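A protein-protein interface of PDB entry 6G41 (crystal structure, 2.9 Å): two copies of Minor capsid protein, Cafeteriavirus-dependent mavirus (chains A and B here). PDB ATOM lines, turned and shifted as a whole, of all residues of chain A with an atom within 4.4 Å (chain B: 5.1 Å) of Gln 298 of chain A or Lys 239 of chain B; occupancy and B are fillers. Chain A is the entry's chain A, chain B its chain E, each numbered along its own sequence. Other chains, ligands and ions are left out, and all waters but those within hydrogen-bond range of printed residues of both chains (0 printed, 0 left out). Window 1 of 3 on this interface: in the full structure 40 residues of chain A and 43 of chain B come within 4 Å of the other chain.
The backbone carbonyl oxygen (O) of Gln 298 of chain A is in hydrogen-bond range of the backbone NH (N) of His 57 of chain A (2.9 Å). The side-chain hydroxyl (OG) of Ser 202 of chain B lies within hydrogen-bond range of a ring nitrogen (ND1) of His 203 of chain B (2.8 Å). The side-chain hydroxyl of Ser 202 of chain B is in hydrogen-bond range of the side-chain amino group of Lys 239 of chain B (3.1 Å). O of Ser 202 of chain B sits at hydrogen-bond distance from N of Tyr 240 of chain B, 3.3 Å away. The side-chain amino group (NZ) of Lys 239 of chain B sits at hydrogen-bond distance from the side-chain hydroxyl (OH) of Tyr 282 of chain B, at 3.3 Å.
Gln 298 of chain A touches just these residues of chain B: Ser 202 (3.1 Å), His 203 (3.6 Å), Lys 239 (3.6 Å) and Tyr 282 (3.8 Å). Lys 239 of chain B touches just these residues of chain A: His 57 (3.2 Å), Leu 252 (3.7 Å), Arg 254 (3.7 Å) and Gln 298 (3.6 Å). Of the printed residues of chain B, Arg 254 of chain A touches Lys 239. Of the printed residues of chain A, Ser 202 of chain B touches Gln 298 (3.1 Å). The nearest printed residue of chain B that does not touch Gln 298 of chain A is Asn 237 of chain B (6.6 Å). The nearest printed residue of chain A that does not touch His 203 of chain B is His 57 of chain A (7.2 Å).
No position is printed for both chains. Of the 10 pairs that touch across the chains among the printed residues, none has its exchanged pair printed and touching as well.
His 57 of chain A touches Lys 239 of chain B. Leu 252 of chain A touches Lys 239 of chain B (CD2 to CG, 3.7 Å). Leu 241 of chain B touches Leu 252 of chain A (CD1 to CD2, 3.9 Å). NH1 of Arg 254 of chain A touches CB of Lys 239 of chain B, at 3.7 Å. Tyr 282 of chain B touches Val 296 of chain A. NE2 of Gln 298 of chain A touches CE1 of His 203 of chain B, at 3.6 Å. NE2 of Gln 298 of chain A touches NZ of Lys 239 of chain B, 3.6 Å away. Tyr 282 of chain B touches Gln 298 of chain A (CD1 to OE1, 3.8 Å).
Of the 8 printed residues of chain B, 5 touch a printed residue of chain A. Printed residues of chain B that touch a printed residue of chain A: Ser 202, His 203, Lys 239, Leu 241 and Tyr 282. Hydrophobic or aromatic side chains of chain B that line the printed part of chain A: His 203, Leu 241 and Tyr 282. Among the printed residues, no Asp or Glu carboxylate lies within 4 Å of a Lys or Arg side-chain nitrogen of the other chain.
A ring nitrogen (NE2) of His 57 of chain A is in hydrogen-bond range of the side-chain hydroxyl (OH) of Tyr 282 of chain B, 3.3 Å away. The side-chain hydroxyl (OG) of Ser 202 of chain B sits at hydrogen-bond distance from the side-chain amide oxygen (OE1) of Gln 298 of chain A, at 3.1 Å.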
ATOM      1  N   GLU A  13      29.087  15.128 -12.351  1.00  0.00           N
ATOM      2  CA  GLU A  13      27.773  15.049 -12.970  1.00  0.00           C
ATOM      3  C   GLU A  13      26.763  15.837 -12.155  1.00  0.00           C
ATOM      4  O   GLU A  13      26.888  15.935 -10.941  1.00  0.00           O
ATOM      5  CB  GLU A  13      27.343  13.583 -13.101  1.00  0.00           C
ATOM      6  CG  GLU A  13      26.131  13.362 -13.988  1.00  0.00           C
ATOM      7  CD  GLU A  13      26.324  13.858 -15.415  1.00  0.00           C
ATOM      8  OE1 GLU A  13      27.146  13.268 -16.155  1.00  0.00           O
ATOM      9  OE2 GLU A  13      25.641  14.839 -15.794  1.00  0.00           O
ATOM     10  N   THR A  14      25.756  16.380 -12.831  1.00  0.00           N
ATOM     11  CA  THR A  14      24.825  17.308 -12.203  1.00  0.00           C
ATOM     12  C   THR A  14      23.461  17.339 -12.914  1.00  0.00           C
ATOM     13  O   THR A  14      23.398  17.144 -14.121  1.00  0.00           O
ATOM     14  CB  THR A  14      25.465  18.719 -12.151  1.00  0.00           C
ATOM     15  OG1 THR A  14      24.608  19.626 -11.448  1.00  0.00           O
ATOM     16  CG2 THR A  14      25.749  19.267 -13.560  1.00  0.00           C
ATOM     17  N   PHE A  56      28.117  13.566  -2.966  1.00  0.00           N
ATOM     18  CA  PHE A  56      26.910  14.036  -3.650  1.00  0.00           C
ATOM     19  C   PHE A  56      26.174  15.108  -2.839  1.00  0.00           C
ATOM     20  O   PHE A  56      26.440  15.315  -1.653  1.00  0.00           O
ATOM     21  CB  PHE A  56      25.975  12.878  -4.065  1.00  0.00           C
ATOM     22  CG  PHE A  56      25.310  12.161  -2.925  1.00  0.00           C
ATOM     23  CD1 PHE A  56      24.168  12.684  -2.318  1.00  0.00           C
ATOM     24  CD2 PHE A  56      25.776  10.927  -2.497  1.00  0.00           C
ATOM     25  CE1 PHE A  56      23.536  12.010  -1.280  1.00  0.00           C
ATOM     26  CE2 PHE A  56      25.148  10.250  -1.459  1.00  0.00           C
ATOM     27  CZ  PHE A  56      24.027  10.791  -0.852  1.00  0.00           C
ATOM     28  N   HIS A  57      25.256  15.791  -3.512  1.00  0.00           N
ATOM     29  CA  HIS A  57      24.438  16.820  -2.893  1.00  0.00           C
ATOM     30  C   HIS A  57      23.039  16.779  -3.506  1.00  0.00           C
ATOM     31  O   HIS A  57      22.886  16.928  -4.713  1.00  0.00           O
ATOM     32  CB  HIS A  57      25.095  18.185  -3.090  1.00  0.00           C
ATOM     33  CG  HIS A  57      24.539  19.267  -2.219  1.00  0.00           C
ATOM     34  ND1 HIS A  57      24.290  19.099  -0.874  1.00  0.00           N
ATOM     35  CD2 HIS A  57      24.207  20.545  -2.500  1.00  0.00           C
ATOM     36  CE1 HIS A  57      23.820  20.224  -0.368  1.00  0.00           C
ATOM     37  NE2 HIS A  57      23.760  21.120  -1.334  1.00  0.00           N
ATOM     38  N   LEU A 252      23.688  16.432   2.109  1.00  0.00           N
ATOM     39  CA  LEU A 252      25.069  16.520   1.668  1.00  0.00           C
ATOM     40  C   LEU A 252      25.837  15.312   2.181  1.00  0.00           C
ATOM     41  O   LEU A 252      25.807  15.025   3.370  1.00  0.00           O
ATOM     42  CB  LEU A 252      25.682  17.803   2.210  1.00  0.00           C
ATOM     43  CG  LEU A 252      27.175  18.043   1.992  1.00  0.00           C
ATOM     44  CD1 LEU A 252      27.546  17.972   0.515  1.00  0.00           C
ATOM     45  CD2 LEU A 252      27.567  19.391   2.584  1.00  0.00           C
ATOM     46  N   ARG A 254      29.771  13.360   1.955  1.00  0.00           N
ATOM     47  CA  ARG A 254      31.195  13.369   1.612  1.00  0.00           C
ATOM     48  C   ARG A 254      31.837  12.171   2.310  1.00  0.00           C
ATOM     49  O   ARG A 254      31.373  11.755   3.371  1.00  0.00           O
ATOM     50  CB  ARG A 254      31.847  14.675   2.056  1.00  0.00           C
ATOM     51  CG  ARG A 254      31.352  15.899   1.295  1.00  0.00           C
ATOM     52  CD  ARG A 254      31.886  17.200   1.878  1.00  0.00           C
ATOM     53  NE  ARG A 254      31.225  17.571   3.135  1.00  0.00           N
ATOM     54  CZ  ARG A 254      31.416  18.717   3.795  1.00  0.00           C
ATOM     55  NH1 ARG A 254      32.254  19.650   3.339  1.00  0.00           N
ATOM     56  NH2 ARG A 254      30.756  18.938   4.924  1.00  0.00           N
ATOM     57  N   VAL A 296      18.390  20.870  -7.290  1.00  0.00           N
ATOM     58  CA  VAL A 296      19.687  20.796  -7.953  1.00  0.00           C
ATOM     59  C   VAL A 296      20.393  19.605  -7.332  1.00  0.00           C
ATOM     60  O   VAL A 296      20.463  19.491  -6.117  1.00  0.00           O
ATOM     61  CB  VAL A 296      20.533  22.070  -7.742  1.00  0.00           C
ATOM     62  CG1 VAL A 296      21.883  21.949  -8.440  1.00  0.00           C
ATOM     63  CG2 VAL A 296      19.793  23.298  -8.256  1.00  0.00           C
ATOM     64  N   ILE A 297      20.916  18.725  -8.174  1.00  0.00           N
ATOM     65  CA  ILE A 297      21.609  17.525  -7.719  1.00  0.00           C
ATOM     66  C   ILE A 297      23.016  17.520  -8.286  1.00  0.00           C
ATOM     67  O   ILE A 297      23.201  17.788  -9.468  1.00  0.00           O
ATOM     68  CB  ILE A 297      20.813  16.267  -8.127  1.00  0.00           C
ATOM     69  CG1 ILE A 297      19.620  16.112  -7.178  1.00  0.00           C
ATOM     70  CG2 ILE A 297      21.663  14.999  -8.095  1.00  0.00           C
ATOM     71  CD1 ILE A 297      18.418  15.501  -7.839  1.00  0.00           C
ATOM     72  N   GLN A 298      23.991  17.224  -7.429  1.00  0.00           N
ATOM     73  CA  GLN A 298      25.398  17.105  -7.811  1.00  0.00           C
ATOM     74  C   GLN A 298      25.944  15.764  -7.372  1.00  0.00           C
ATOM     75  O   GLN A 298      25.486  15.198  -6.386  1.00  0.00           O
ATOM     76  CB  GLN A 298      26.214  18.198  -7.154  1.00  0.00           C
ATOM     77  CG  GLN A 298      25.995  19.566  -7.759  1.00  0.00           C
ATOM     78  CD  GLN A 298      26.496  20.704  -6.888  1.00  0.00           C
ATOM     79  OE1 GLN A 298      26.073  21.851  -7.073  1.00  0.00           O
ATOM     80  NE2 GLN A 298      27.392  20.411  -5.939  1.00  0.00           N
ATOM     81  N   LEU A 299      26.960  15.294  -8.087  1.00  0.00           N
ATOM     82  CA  LEU A 299      27.435  13.921  -7.972  1.00  0.00           C
ATOM     83  C   LEU A 299      28.869  13.821  -8.491  1.00  0.00           C
ATOM     84  O   LEU A 299      29.193  14.386  -9.536  1.00  0.00           O
ATOM     85  CB  LEU A 299      26.511  13.021  -8.796  1.00  0.00           C
ATOM     86  CG  LEU A 299      26.778  11.525  -8.909  1.00  0.00           C
ATOM     87  CD1 LEU A 299      26.801  10.849  -7.547  1.00  0.00           C
ATOM     88  CD2 LEU A 299      25.697  10.922  -9.785  1.00  0.00           C
ATOM     89  N   SER B 202      27.781  27.195  -4.132  1.00  0.00           N
ATOM     90  CA  SER B 202      27.874  25.737  -3.989  1.00  0.00           C
ATOM     91  C   SER B 202      29.240  25.313  -3.461  1.00  0.00           C
ATOM     92  O   SER B 202      29.339  24.753  -2.367  1.00  0.00           O
ATOM     93  CB  SER B 202      27.576  25.026  -5.313  1.00  0.00           C
ATOM     94  OG  SER B 202      27.719  23.621  -5.171  1.00  0.00           O
ATOM     95  N   HIS B 203      30.286  25.563  -4.246  1.00  0.00           N
ATOM     96  CA  HIS B 203      31.657  25.196  -3.851  1.00  0.00           C
ATOM     97  C   HIS B 203      32.696  26.203  -4.332  1.00  0.00           C
ATOM     98  O   HIS B 203      32.397  27.077  -5.143  1.00  0.00           O
ATOM     99  CB  HIS B 203      32.017  23.754  -4.276  1.00  0.00           C
ATOM    100  CG  HIS B 203      31.490  23.356  -5.619  1.00  0.00           C
ATOM    101  ND1 HIS B 203      30.266  22.744  -5.786  1.00  0.00           N
ATOM    102  CD2 HIS B 203      32.027  23.470  -6.858  1.00  0.00           C
ATOM    103  CE1 HIS B 203      30.064  22.515  -7.072  1.00  0.00           C
ATOM    104  NE2 HIS B 203      31.119  22.942  -7.744  1.00  0.00           N
ATOM    105  N   ASN B 237      38.187  20.900  -4.351  1.00  0.00           N
ATOM    106  CA  ASN B 237      36.755  21.138  -4.518  1.00  0.00           C
ATOM    107  C   ASN B 237      36.129  21.239  -3.122  1.00  0.00           C
ATOM    108  O   ASN B 237      35.711  20.240  -2.554  1.00  0.00           O
ATOM    109  CB  ASN B 237      36.160  19.978  -5.342  1.00  0.00           C
ATOM    110  CG  ASN B 237      34.686  20.160  -5.656  1.00  0.00           C
ATOM    111  OD1 ASN B 237      34.276  21.192  -6.189  1.00  0.00           O
ATOM    112  ND2 ASN B 237      33.880  19.139  -5.354  1.00  0.00           N
ATOM    113  N   TYR B 238      36.102  22.453  -2.572  1.00  0.00           N
ATOM    114  CA  TYR B 238      35.664  22.699  -1.191  1.00  0.00           C
ATOM    115  C   TYR B 238      34.181  23.026  -1.130  1.00  0.00           C
ATOM    116  O   TYR B 238      33.755  24.045  -1.669  1.00  0.00           O
ATOM    117  CB  TYR B 238      36.453  23.867  -0.598  1.00  0.00           C
ATOM    118  CG  TYR B 238      36.034  24.272   0.805  1.00  0.00           C
ATOM    119  CD1 TYR B 238      36.455  23.544   1.920  1.00  0.00           C
ATOM    120  CD2 TYR B 238      35.230  25.391   1.018  1.00  0.00           C
ATOM    121  CE1 TYR B 238      36.083  23.916   3.205  1.00  0.00           C
ATOM    122  CE2 TYR B 238      34.849  25.773   2.299  1.00  0.00           C
ATOM    123  CZ  TYR B 238      35.280  25.036   3.394  1.00  0.00           C
ATOM    124  OH  TYR B 238      34.904  25.418   4.669  1.00  0.00           O
ATOM    125  N   LYS B 239      33.408  22.183  -0.445  1.00  0.00           N
ATOM    126  CA  LYS B 239      31.970  22.407  -0.280  1.00  0.00           C
ATOM    127  C   LYS B 239      31.713  23.470   0.784  1.00  0.00           C
ATOM    128  O   LYS B 239      32.017  23.264   1.955  1.00  0.00           O
ATOM    129  CB  LYS B 239      31.256  21.104   0.092  1.00  0.00           C
ATOM    130  CG  LYS B 239      29.733  21.195   0.123  1.00  0.00           C
ATOM    131  CD  LYS B 239      29.138  21.290  -1.270  1.00  0.00           C
ATOM    132  CE  LYS B 239      27.723  21.836  -1.246  1.00  0.00           C
ATOM    133  NZ  LYS B 239      27.147  21.877  -2.619  1.00  0.00           N
ATOM    134  N   TYR B 240      31.143  24.594   0.357  1.00  0.00           N
ATOM    135  CA  TYR B 240      30.838  25.725   1.232  1.00  0.00           C
ATOM    136  C   TYR B 240      29.392  25.680   1.739  1.00  0.00           C
ATOM    137  O   TYR B 240      28.470  25.353   0.993  1.00  0.00           O
ATOM    138  CB  TYR B 240      31.081  27.040   0.489  1.00  0.00           C
ATOM    139  CG  TYR B 240      30.775  28.278   1.303  1.00  0.00           C
ATOM    140  CD1 TYR B 240      31.631  28.697   2.323  1.00  0.00           C
ATOM    141  CD2 TYR B 240      29.630  29.029   1.059  1.00  0.00           C
ATOM    142  CE1 TYR B 240      31.357  29.831   3.074  1.00  0.00           C
ATOM    143  CE2 TYR B 240      29.344  30.165   1.800  1.00  0.00           C
ATOM    144  CZ  TYR B 240      30.210  30.565   2.810  1.00  0.00           C
ATOM    145  OH  TYR B 240      29.929  31.694   3.552  1.00  0.00           O
ATOM    146  N   LEU B 241      29.216  26.033   3.011  1.00  0.00           N
ATOM    147  CA  LEU B 241      27.913  26.038   3.680  1.00  0.00           C
ATOM    148  C   LEU B 241      27.757  27.331   4.464  1.00  0.00           C
ATOM    149  O   LEU B 241      28.587  27.637   5.323  1.00  0.00           O
ATOM    150  CB  LEU B 241      27.796  24.847   4.633  1.00  0.00           C
ATOM    151  CG  LEU B 241      27.826  23.462   3.985  1.00  0.00           C
ATOM    152  CD1 LEU B 241      28.099  22.397   5.034  1.00  0.00           C
ATOM    153  CD2 LEU B 241      26.521  23.180   3.247  1.00  0.00           C
ATOM    154  N   TYR B 282      25.084  27.335  -7.560  1.00  0.00           N
ATOM    155  CA  TYR B 282      24.165  26.199  -7.785  1.00  0.00           C
ATOM    156  C   TYR B 282      23.636  26.106  -9.213  1.00  0.00           C
ATOM    157  O   TYR B 282      23.414  25.006  -9.720  1.00  0.00           O
ATOM    158  CB  TYR B 282      23.013  26.207  -6.760  1.00  0.00           C
ATOM    159  CG  TYR B 282      23.482  25.688  -5.431  1.00  0.00           C
ATOM    160  CD1 TYR B 282      23.853  24.354  -5.293  1.00  0.00           C
ATOM    161  CD2 TYR B 282      23.621  26.529  -4.333  1.00  0.00           C
ATOM    162  CE1 TYR B 282      24.331  23.861  -4.096  1.00  0.00           C
ATOM    163  CE2 TYR B 282      24.098  26.043  -3.124  1.00  0.00           C
ATOM    164  CZ  TYR B 282      24.450  24.703  -3.014  1.00  0.00           C
ATOM    165  OH  TYR B 282      24.936  24.192  -1.839  1.00  0.00           O
